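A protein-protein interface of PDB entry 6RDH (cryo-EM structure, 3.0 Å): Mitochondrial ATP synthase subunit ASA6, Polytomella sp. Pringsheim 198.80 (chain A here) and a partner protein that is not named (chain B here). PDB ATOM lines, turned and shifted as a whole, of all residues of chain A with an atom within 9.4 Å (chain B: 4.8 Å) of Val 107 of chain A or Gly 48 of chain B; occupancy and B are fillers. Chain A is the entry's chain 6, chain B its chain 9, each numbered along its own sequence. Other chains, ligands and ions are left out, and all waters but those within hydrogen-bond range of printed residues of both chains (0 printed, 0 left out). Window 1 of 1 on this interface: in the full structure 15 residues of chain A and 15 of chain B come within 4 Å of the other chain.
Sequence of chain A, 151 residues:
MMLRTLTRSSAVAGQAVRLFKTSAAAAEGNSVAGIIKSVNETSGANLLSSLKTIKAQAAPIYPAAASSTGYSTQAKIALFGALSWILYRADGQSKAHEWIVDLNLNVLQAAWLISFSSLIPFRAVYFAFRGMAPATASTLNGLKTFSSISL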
ATOM      1  N   GLN A  93     -16.064 -17.131  -5.884  1.00  0.00           N
ATOM      2  CA  GLN A  93     -15.458 -18.046  -4.924  1.00  0.00           C
ATOM      3  C   GLN A  93     -16.258 -18.111  -3.645  1.00  0.00           C
ATOM      4  O   GLN A  93     -16.289 -19.150  -2.980  1.00  0.00           O
ATOM      5  CB  GLN A  93     -14.031 -17.635  -4.587  1.00  0.00           C
ATOM      6  CG  GLN A  93     -12.995 -18.037  -5.580  1.00  0.00           C
ATOM      7  CD  GLN A  93     -11.626 -17.643  -5.126  1.00  0.00           C
ATOM      8  OE1 GLN A  93     -11.471 -16.939  -4.138  1.00  0.00           O
ATOM      9  NE2 GLN A  93     -10.612 -18.133  -5.818  1.00  0.00           N
ATOM     10  N   ILE A 100     -15.183 -20.986   2.119  1.00  0.00           N
ATOM     11  CA  ILE A 100     -14.140 -20.522   3.021  1.00  0.00           C
ATOM     12  C   ILE A 100     -12.825 -21.197   2.671  1.00  0.00           C
ATOM     13  O   ILE A 100     -11.751 -20.606   2.822  1.00  0.00           O
ATOM     14  CB  ILE A 100     -14.572 -20.752   4.481  1.00  0.00           C
ATOM     15  CG1 ILE A 100     -13.561 -20.174   5.465  1.00  0.00           C
ATOM     16  CG2 ILE A 100     -14.826 -22.203   4.759  1.00  0.00           C
ATOM     17  CD1 ILE A 100     -13.412 -18.695   5.369  1.00  0.00           C
ATOM     18  N   VAL A 101     -12.894 -22.389   2.087  1.00  0.00           N
ATOM     19  CA  VAL A 101     -11.702 -23.073   1.616  1.00  0.00           C
ATOM     20  C   VAL A 101     -11.093 -22.331   0.430  1.00  0.00           C
ATOM     21  O   VAL A 101      -9.872 -22.178   0.346  1.00  0.00           O
ATOM     22  CB  VAL A 101     -12.073 -24.530   1.296  1.00  0.00           C
ATOM     23  CG1 VAL A 101     -11.042 -25.198   0.464  1.00  0.00           C
ATOM     24  CG2 VAL A 101     -12.309 -25.296   2.575  1.00  0.00           C
ATOM     25  N   ASP A 102     -11.931 -21.778  -0.454  1.00  0.00           N
ATOM     26  CA  ASP A 102     -11.422 -20.977  -1.568  1.00  0.00           C
ATOM     27  C   ASP A 102     -10.827 -19.660  -1.092  1.00  0.00           C
ATOM     28  O   ASP A 102      -9.759 -19.245  -1.570  1.00  0.00           O
ATOM     29  CB  ASP A 102     -12.530 -20.697  -2.576  1.00  0.00           C
ATOM     30  CG  ASP A 102     -13.062 -21.948  -3.215  1.00  0.00           C
ATOM     31  OD1 ASP A 102     -12.770 -23.037  -2.696  1.00  0.00           O
ATOM     32  OD2 ASP A 102     -13.763 -21.847  -4.242  1.00  0.00           O
ATOM     33  N   LEU A 103     -11.503 -18.987  -0.155  1.00  0.00           N
ATOM     34  CA  LEU A 103     -10.987 -17.722   0.357  1.00  0.00           C
ATOM     35  C   LEU A 103      -9.688 -17.908   1.119  1.00  0.00           C
ATOM     36  O   LEU A 103      -8.865 -16.993   1.165  1.00  0.00           O
ATOM     37  CB  LEU A 103     -12.010 -17.047   1.256  1.00  0.00           C
ATOM     38  CG  LEU A 103     -13.356 -16.713   0.635  1.00  0.00           C
ATOM     39  CD1 LEU A 103     -14.191 -16.041   1.682  1.00  0.00           C
ATOM     40  CD2 LEU A 103     -13.207 -15.840  -0.586  1.00  0.00           C
ATOM     41  N   ASN A 104      -9.471 -19.080   1.698  1.00  0.00           N
ATOM     42  CA  ASN A 104      -8.193 -19.349   2.331  1.00  0.00           C
ATOM     43  C   ASN A 104      -7.144 -19.879   1.365  1.00  0.00           C
ATOM     44  O   ASN A 104      -5.946 -19.749   1.636  1.00  0.00           O
ATOM     45  CB  ASN A 104      -8.426 -20.306   3.484  1.00  0.00           C
ATOM     46  CG  ASN A 104      -9.113 -19.629   4.633  1.00  0.00           C
ATOM     47  OD1 ASN A 104     -10.172 -19.038   4.488  1.00  0.00           O
ATOM     48  ND2 ASN A 104      -8.524 -19.720   5.783  1.00  0.00           N
ATOM     49  N   LEU A 105      -7.556 -20.441   0.232  1.00  0.00           N
ATOM     50  CA  LEU A 105      -6.581 -20.785  -0.794  1.00  0.00           C
ATOM     51  C   LEU A 105      -6.008 -19.548  -1.457  1.00  0.00           C
ATOM     52  O   LEU A 105      -4.847 -19.561  -1.882  1.00  0.00           O
ATOM     53  CB  LEU A 105      -7.212 -21.698  -1.832  1.00  0.00           C
ATOM     54  CG  LEU A 105      -7.232 -23.157  -1.404  1.00  0.00           C
ATOM     55  CD1 LEU A 105      -7.788 -24.006  -2.505  1.00  0.00           C
ATOM     56  CD2 LEU A 105      -5.850 -23.604  -1.056  1.00  0.00           C
ATOM     57  N   ASN A 106      -6.797 -18.476  -1.548  1.00  0.00           N
ATOM     58  CA  ASN A 106      -6.250 -17.201  -2.009  1.00  0.00           C
ATOM     59  C   ASN A 106      -5.159 -16.692  -1.071  1.00  0.00           C
ATOM     60  O   ASN A 106      -4.154 -16.134  -1.521  1.00  0.00           O
ATOM     61  CB  ASN A 106      -7.356 -16.166  -2.138  1.00  0.00           C
ATOM     62  CG  ASN A 106      -8.417 -16.582  -3.104  1.00  0.00           C
ATOM     63  OD1 ASN A 106      -8.148 -17.275  -4.075  1.00  0.00           O
ATOM     64  ND2 ASN A 106      -9.642 -16.167  -2.843  1.00  0.00           N
ATOM     65  N   VAL A 107      -5.325 -16.912   0.230  1.00  0.00           N
ATOM     66  CA  VAL A 107      -4.299 -16.551   1.202  1.00  0.00           C
ATOM     67  C   VAL A 107      -3.074 -17.436   1.042  1.00  0.00           C
ATOM     68  O   VAL A 107      -1.935 -16.958   1.086  1.00  0.00           O
ATOM     69  CB  VAL A 107      -4.887 -16.634   2.620  1.00  0.00           C
ATOM     70  CG1 VAL A 107      -3.814 -16.548   3.672  1.00  0.00           C
ATOM     71  CG2 VAL A 107      -5.892 -15.535   2.821  1.00  0.00           C
ATOM     72  N   LEU A 108      -3.292 -18.735   0.821  1.00  0.00           N
ATOM     73  CA  LEU A 108      -2.186 -19.676   0.660  1.00  0.00           C
ATOM     74  C   LEU A 108      -1.371 -19.398  -0.588  1.00  0.00           C
ATOM     75  O   LEU A 108      -0.179 -19.707  -0.629  1.00  0.00           O
ATOM     76  CB  LEU A 108      -2.718 -21.097   0.613  1.00  0.00           C
ATOM     77  CG  LEU A 108      -2.731 -21.791   1.958  1.00  0.00           C
ATOM     78  CD1 LEU A 108      -3.389 -23.114   1.797  1.00  0.00           C
ATOM     79  CD2 LEU A 108      -1.318 -21.965   2.437  1.00  0.00           C
ATOM     80  N   GLN A 109      -1.987 -18.819  -1.609  1.00  0.00           N
ATOM     81  CA  GLN A 109      -1.258 -18.455  -2.814  1.00  0.00           C
ATOM     82  C   GLN A 109      -0.589 -17.087  -2.718  1.00  0.00           C
ATOM     83  O   GLN A 109       0.556 -16.921  -3.166  1.00  0.00           O
ATOM     84  CB  GLN A 109      -2.210 -18.509  -4.002  1.00  0.00           C
ATOM     85  CG  GLN A 109      -2.628 -19.916  -4.308  1.00  0.00           C
ATOM     86  CD  GLN A 109      -3.911 -19.987  -5.061  1.00  0.00           C
ATOM     87  OE1 GLN A 109      -4.567 -18.982  -5.279  1.00  0.00           O
ATOM     88  NE2 GLN A 109      -4.285 -21.185  -5.469  1.00  0.00           N
ATOM     89  N   ALA A 110      -1.273 -16.100  -2.128  1.00  0.00           N
ATOM     90  CA  ALA A 110      -0.667 -14.789  -1.940  1.00  0.00           C
ATOM     91  C   ALA A 110       0.498 -14.841  -0.966  1.00  0.00           C
ATOM     92  O   ALA A 110       1.406 -14.008  -1.044  1.00  0.00           O
ATOM     93  CB  ALA A 110      -1.715 -13.796  -1.459  1.00  0.00           C
ATOM     94  N   ALA A 111       0.505 -15.825  -0.065  1.00  0.00           N
ATOM     95  CA  ALA A 111       1.648 -16.025   0.813  1.00  0.00           C
ATOM     96  C   ALA A 111       2.887 -16.407   0.025  1.00  0.00           C
ATOM     97  O   ALA A 111       3.988 -15.944   0.330  1.00  0.00           O
ATOM     98  CB  ALA A 111       1.324 -17.093   1.848  1.00  0.00           C
ATOM     99  N   TRP A 112       2.729 -17.221  -1.016  1.00  0.00           N
ATOM    100  CA  TRP A 112       3.892 -17.606  -1.809  1.00  0.00           C
ATOM    101  C   TRP A 112       4.298 -16.523  -2.781  1.00  0.00           C
ATOM    102  O   TRP A 112       5.467 -16.449  -3.148  1.00  0.00           O
ATOM    103  CB  TRP A 112       3.629 -18.888  -2.576  1.00  0.00           C
ATOM    104  CG  TRP A 112       4.108 -20.061  -1.874  1.00  0.00           C
ATOM    105  CD1 TRP A 112       3.360 -20.951  -1.206  1.00  0.00           C
ATOM    106  CD2 TRP A 112       5.462 -20.474  -1.724  1.00  0.00           C
ATOM    107  NE1 TRP A 112       4.148 -21.921  -0.658  1.00  0.00           N
ATOM    108  CE2 TRP A 112       5.451 -21.645  -0.961  1.00  0.00           C
ATOM    109  CE3 TRP A 112       6.682 -19.968  -2.160  1.00  0.00           C
ATOM    110  CZ2 TRP A 112       6.608 -22.325  -0.626  1.00  0.00           C
ATOM    111  CZ3 TRP A 112       7.830 -20.644  -1.832  1.00  0.00           C
ATOM    112  CH2 TRP A 112       7.788 -21.809  -1.071  1.00  0.00           C
ATOM    113  N   LEU A 113       3.354 -15.691  -3.213  1.00  0.00           N
ATOM    114  CA  LEU A 113       3.725 -14.485  -3.953  1.00  0.00           C
ATOM    115  C   LEU A 113       4.583 -13.560  -3.096  1.00  0.00           C
ATOM    116  O   LEU A 113       5.614 -13.047  -3.552  1.00  0.00           O
ATOM    117  CB  LEU A 113       2.473 -13.754  -4.422  1.00  0.00           C
ATOM    118  CG  LEU A 113       2.011 -13.926  -5.859  1.00  0.00           C
ATOM    119  CD1 LEU A 113       1.661 -15.350  -6.126  1.00  0.00           C
ATOM    120  CD2 LEU A 113       0.818 -13.049  -6.109  1.00  0.00           C
ATOM    121  N   ILE A 114       4.180 -13.364  -1.838  1.00  0.00           N
ATOM    122  CA  ILE A 114       4.939 -12.552  -0.888  1.00  0.00           C
ATOM    123  C   ILE A 114       6.300 -13.183  -0.602  1.00  0.00           C
ATOM    124  O   ILE A 114       7.315 -12.486  -0.498  1.00  0.00           O
ATOM    125  CB  ILE A 114       4.094 -12.365   0.389  1.00  0.00           C
ATOM    126  CG1 ILE A 114       3.022 -11.309   0.160  1.00  0.00           C
ATOM    127  CG2 ILE A 114       4.923 -12.016   1.601  1.00  0.00           C
ATOM    128  CD1 ILE A 114       2.069 -11.183   1.297  1.00  0.00           C
ATOM    129  N   SER A 115       6.350 -14.509  -0.515  1.00  0.00           N
ATOM    130  CA  SER A 115       7.610 -15.193  -0.262  1.00  0.00           C
ATOM    131  C   SER A 115       8.544 -15.163  -1.463  1.00  0.00           C
ATOM    132  O   SER A 115       9.760 -15.090  -1.284  1.00  0.00           O
ATOM    133  CB  SER A 115       7.347 -16.635   0.142  1.00  0.00           C
ATOM    134  OG  SER A 115       8.560 -17.330   0.332  1.00  0.00           O
ATOM    135  N   PHE B  44       1.821 -15.475   8.086  1.00  0.00           N
ATOM    136  CA  PHE B  44       0.842 -14.859   7.199  1.00  0.00           C
ATOM    137  C   PHE B  44      -0.305 -15.812   6.922  1.00  0.00           C
ATOM    138  O   PHE B  44      -1.465 -15.394   6.866  1.00  0.00           O
ATOM    139  CB  PHE B  44       1.516 -14.437   5.894  1.00  0.00           C
ATOM    140  CG  PHE B  44       0.611 -13.718   4.933  1.00  0.00           C
ATOM    141  CD1 PHE B  44       0.380 -12.367   5.061  1.00  0.00           C
ATOM    142  CD2 PHE B  44       0.014 -14.390   3.883  1.00  0.00           C
ATOM    143  CE1 PHE B  44      -0.440 -11.702   4.169  1.00  0.00           C
ATOM    144  CE2 PHE B  44      -0.810 -13.735   2.996  1.00  0.00           C
ATOM    145  CZ  PHE B  44      -1.033 -12.390   3.137  1.00  0.00           C
ATOM    146  N   VAL B  45      -0.004 -17.102   6.782  1.00  0.00           N
ATOM    147  CA  VAL B  45      -1.061 -18.078   6.536  1.00  0.00           C
ATOM    148  C   VAL B  45      -1.939 -18.246   7.774  1.00  0.00           C
ATOM    149  O   VAL B  45      -3.167 -18.309   7.667  1.00  0.00           O
ATOM    150  CB  VAL B  45      -0.460 -19.416   6.066  1.00  0.00           C
ATOM    151  CG1 VAL B  45      -1.533 -20.460   5.883  1.00  0.00           C
ATOM    152  CG2 VAL B  45       0.262 -19.226   4.766  1.00  0.00           C
ATOM    153  N   MET B  46      -1.337 -18.279   8.967  1.00  0.00           N
ATOM    154  CA  MET B  46      -2.127 -18.429  10.189  1.00  0.00           C
ATOM    155  C   MET B  46      -2.955 -17.184  10.484  1.00  0.00           C
ATOM    156  O   MET B  46      -4.103 -17.291  10.934  1.00  0.00           O
ATOM    157  CB  MET B  46      -1.216 -18.760  11.365  1.00  0.00           C
ATOM    158  CG  MET B  46      -0.671 -20.172  11.324  1.00  0.00           C
ATOM    159  SD  MET B  46      -0.010 -20.716  12.906  1.00  0.00           S
ATOM    160  CE  MET B  46       0.980 -19.301  13.362  1.00  0.00           C
ATOM    161  N   VAL B  47      -2.404 -15.998  10.213  1.00  0.00           N
ATOM    162  CA  VAL B  47      -3.173 -14.764  10.324  1.00  0.00           C
ATOM    163  C   VAL B  47      -4.322 -14.759   9.324  1.00  0.00           C
ATOM    164  O   VAL B  47      -5.441 -14.360   9.655  1.00  0.00           O
ATOM    165  CB  VAL B  47      -2.240 -13.548  10.153  1.00  0.00           C
ATOM    166  CG1 VAL B  47      -3.006 -12.282   9.849  1.00  0.00           C
ATOM    167  CG2 VAL B  47      -1.442 -13.340  11.414  1.00  0.00           C
ATOM    168  N   GLY B  48      -4.087 -15.272   8.116  1.00  0.00           N
ATOM    169  CA  GLY B  48      -5.146 -15.308   7.122  1.00  0.00           C
ATOM    170  C   GLY B  48      -6.260 -16.272   7.470  1.00  0.00           C
ATOM    171  O   GLY B  48      -7.439 -15.948   7.301  1.00  0.00           O
ATOM    172  N   VAL B  49      -5.910 -17.449   7.997  1.00  0.00           N
ATOM    173  CA  VAL B  49      -6.952 -18.407   8.359  1.00  0.00           C
ATOM    174  C   VAL B  49      -7.728 -17.917   9.577  1.00  0.00           C
ATOM    175  O   VAL B  49      -8.958 -18.054   9.623  1.00  0.00           O
ATOM    176  CB  VAL B  49      -6.395 -19.842   8.556  1.00  0.00           C
ATOM    177  CG1 VAL B  49      -5.670 -20.329   7.313  1.00  0.00           C
ATOM    178  CG2 VAL B  49      -5.501 -19.993   9.758  1.00  0.00           C
ATOM    179  N   ASN B  50      -7.062 -17.236  10.518  1.00  0.00           N
ATOM    180  CA  ASN B  50      -7.767 -16.740  11.689  1.00  0.00           C
ATOM    181  C   ASN B  50      -8.658 -15.557  11.341  1.00  0.00           C
ATOM    182  O   ASN B  50      -9.787 -15.470  11.830  1.00  0.00           O
ATOM    183  CB  ASN B  50      -6.767 -16.378  12.779  1.00  0.00           C
ATOM    184  CG  ASN B  50      -6.224 -17.599  13.495  1.00  0.00           C
ATOM    185  OD1 ASN B  50      -6.840 -18.663  13.473  1.00  0.00           O
ATOM    186  ND2 ASN B  50      -5.077 -17.451  14.142  1.00  0.00           N
ATOM    187  N   VAL B  51      -8.196 -14.671  10.456  1.00  0.00           N
ATOM    188  CA  VAL B  51      -8.987 -13.509  10.066  1.00  0.00           C
ATOM    189  C   VAL B  51     -10.189 -13.928   9.230  1.00  0.00           C
ATOM    190  O   VAL B  51     -11.305 -13.439   9.442  1.00  0.00           O
ATOM    191  CB  VAL B  51      -8.094 -12.487   9.336  1.00  0.00           C
ATOM    192  CG1 VAL B  51      -8.913 -11.496   8.534  1.00  0.00           C
ATOM    193  CG2 VAL B  51      -7.243 -11.738  10.338  1.00  0.00           C
ATOM    194  N   LEU B  52     -10.008 -14.872   8.309  1.00  0.00           N
ATOM    195  CA  LEU B  52     -11.138 -15.302   7.496  1.00  0.00           C
ATOM    196  C   LEU B  52     -12.090 -16.219   8.237  1.00  0.00           C
ATOM    197  O   LEU B  52     -13.243 -16.350   7.820  1.00  0.00           O
ATOM    198  CB  LEU B  52     -10.646 -16.001   6.237  1.00  0.00           C
ATOM    199  CG  LEU B  52      -9.975 -15.046   5.272  1.00  0.00           C
ATOM    200  CD1 LEU B  52      -9.320 -15.857   4.225  1.00  0.00           C
ATOM    201  CD2 LEU B  52     -11.014 -14.130   4.663  1.00  0.00           C
ATOM    202  N   LEU B  53     -11.648 -16.865   9.310  1.00  0.00           N
ATOM    203  CA  LEU B  53     -12.612 -17.571  10.136  1.00  0.00           C
ATOM    204  C   LEU B  53     -13.368 -16.607  11.037  1.00  0.00           C
ATOM    205  O   LEU B  53     -14.582 -16.744  11.218  1.00  0.00           O
ATOM    206  CB  LEU B  53     -11.909 -18.638  10.965  1.00  0.00           C
ATOM    207  CG  LEU B  53     -11.766 -20.022  10.349  1.00  0.00           C
ATOM    208  CD1 LEU B  53     -11.080 -20.928  11.332  1.00  0.00           C
ATOM    209  CD2 LEU B  53     -13.115 -20.573   9.980  1.00  0.00           C
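The backbone carbonyl oxygen (O) of Ile 100 of chain A lies close to the side-chain amide oxygen (OD1) of Asn 104 of chain A.
Of the printed residues of chain B, Val 107 of chain A touches Phe 44 (3.9 Å), Gly 48 (3.9 Å) and Leu 52 (3.7 Å).
Gly 48 of chain B touches just one residue of chain A: Val 107.
Val 45 of chain B touches just these residues of chain A: Leu 108 and Ala 111.
Val 47 of chain B touches none of the printed residues of chain A.
Of chain A, only Asn 104 comes within 4 Å of Val 49 of chain B.
No residue of chain A comes within 4 Å of Val 51 of chain B.
Printed residues of chain A within 4 Å of Leu 52 of chain B: Ile 100 (3.4 Å), Leu 103 (3.3 Å), Asn 104 (3.3 Å) and Val 107 (3.7 Å).
Of the printed residues of chain B, Leu 108 of chain A touches Val 45.
Printed residues of chain B within 4 Å of Ala 111 of chain A: Phe 44 and Val 45.
Of the printed residues of chain B, Asn 104 of chain A touches Val 49 (3.3 Å) and Leu 52 (3.3 Å).
The nearest residue of chain B that does not touch Val 107 of chain A is Val 45 of chain B (4.3 Å).
The nearest printed residue of chain A that does not touch Phe 44 of chain B is Ala 110 of chain A (4.3 Å).
Among the printed residues, pairs that only touch across the chains: Asn 104 of chain A with Val 49 of chain B (3.3 Å), Leu 103 of chain A with Leu 52 of chain B (3.3 Å), Asn 104 of chain A with Leu 52 of chain B (3.3 Å), Ile 100 of chain A with Leu 52 of chain B (3.4 Å), Ala 111 of chain A with Phe 44 of chain B (3.6 Å), Val 107 of chain A with Leu 52 of chain B (3.7 Å), Leu 108 of chain A with Val 45 of chain B (3.8 Å), Ala 111 of chain A with Val 45 of chain B (3.8 Å), Ile 114 of chain A with Phe 44 of chain B (3.8 Å), Val 107 of chain A with Gly 48 of chain B (3.9 Å) and Val 107 of chain A with Phe 44 of chain B (3.9 Å).
Of the 17 printed residues of chain A, 7 touch a printed residue of chain B.
Hydrophobic or aromatic side chains of chain A that line the printed part of chain B: Ile 100, Val 107, Leu 108, Ala 111 and Ile 114.
Of the 10 printed residues of chain B, 5 touch a printed residue of chain A.
Among the printed residues, no Asp or Glu carboxylate lies within 4 Å of a Lys or Arg side-chain nitrogen of the other chain.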
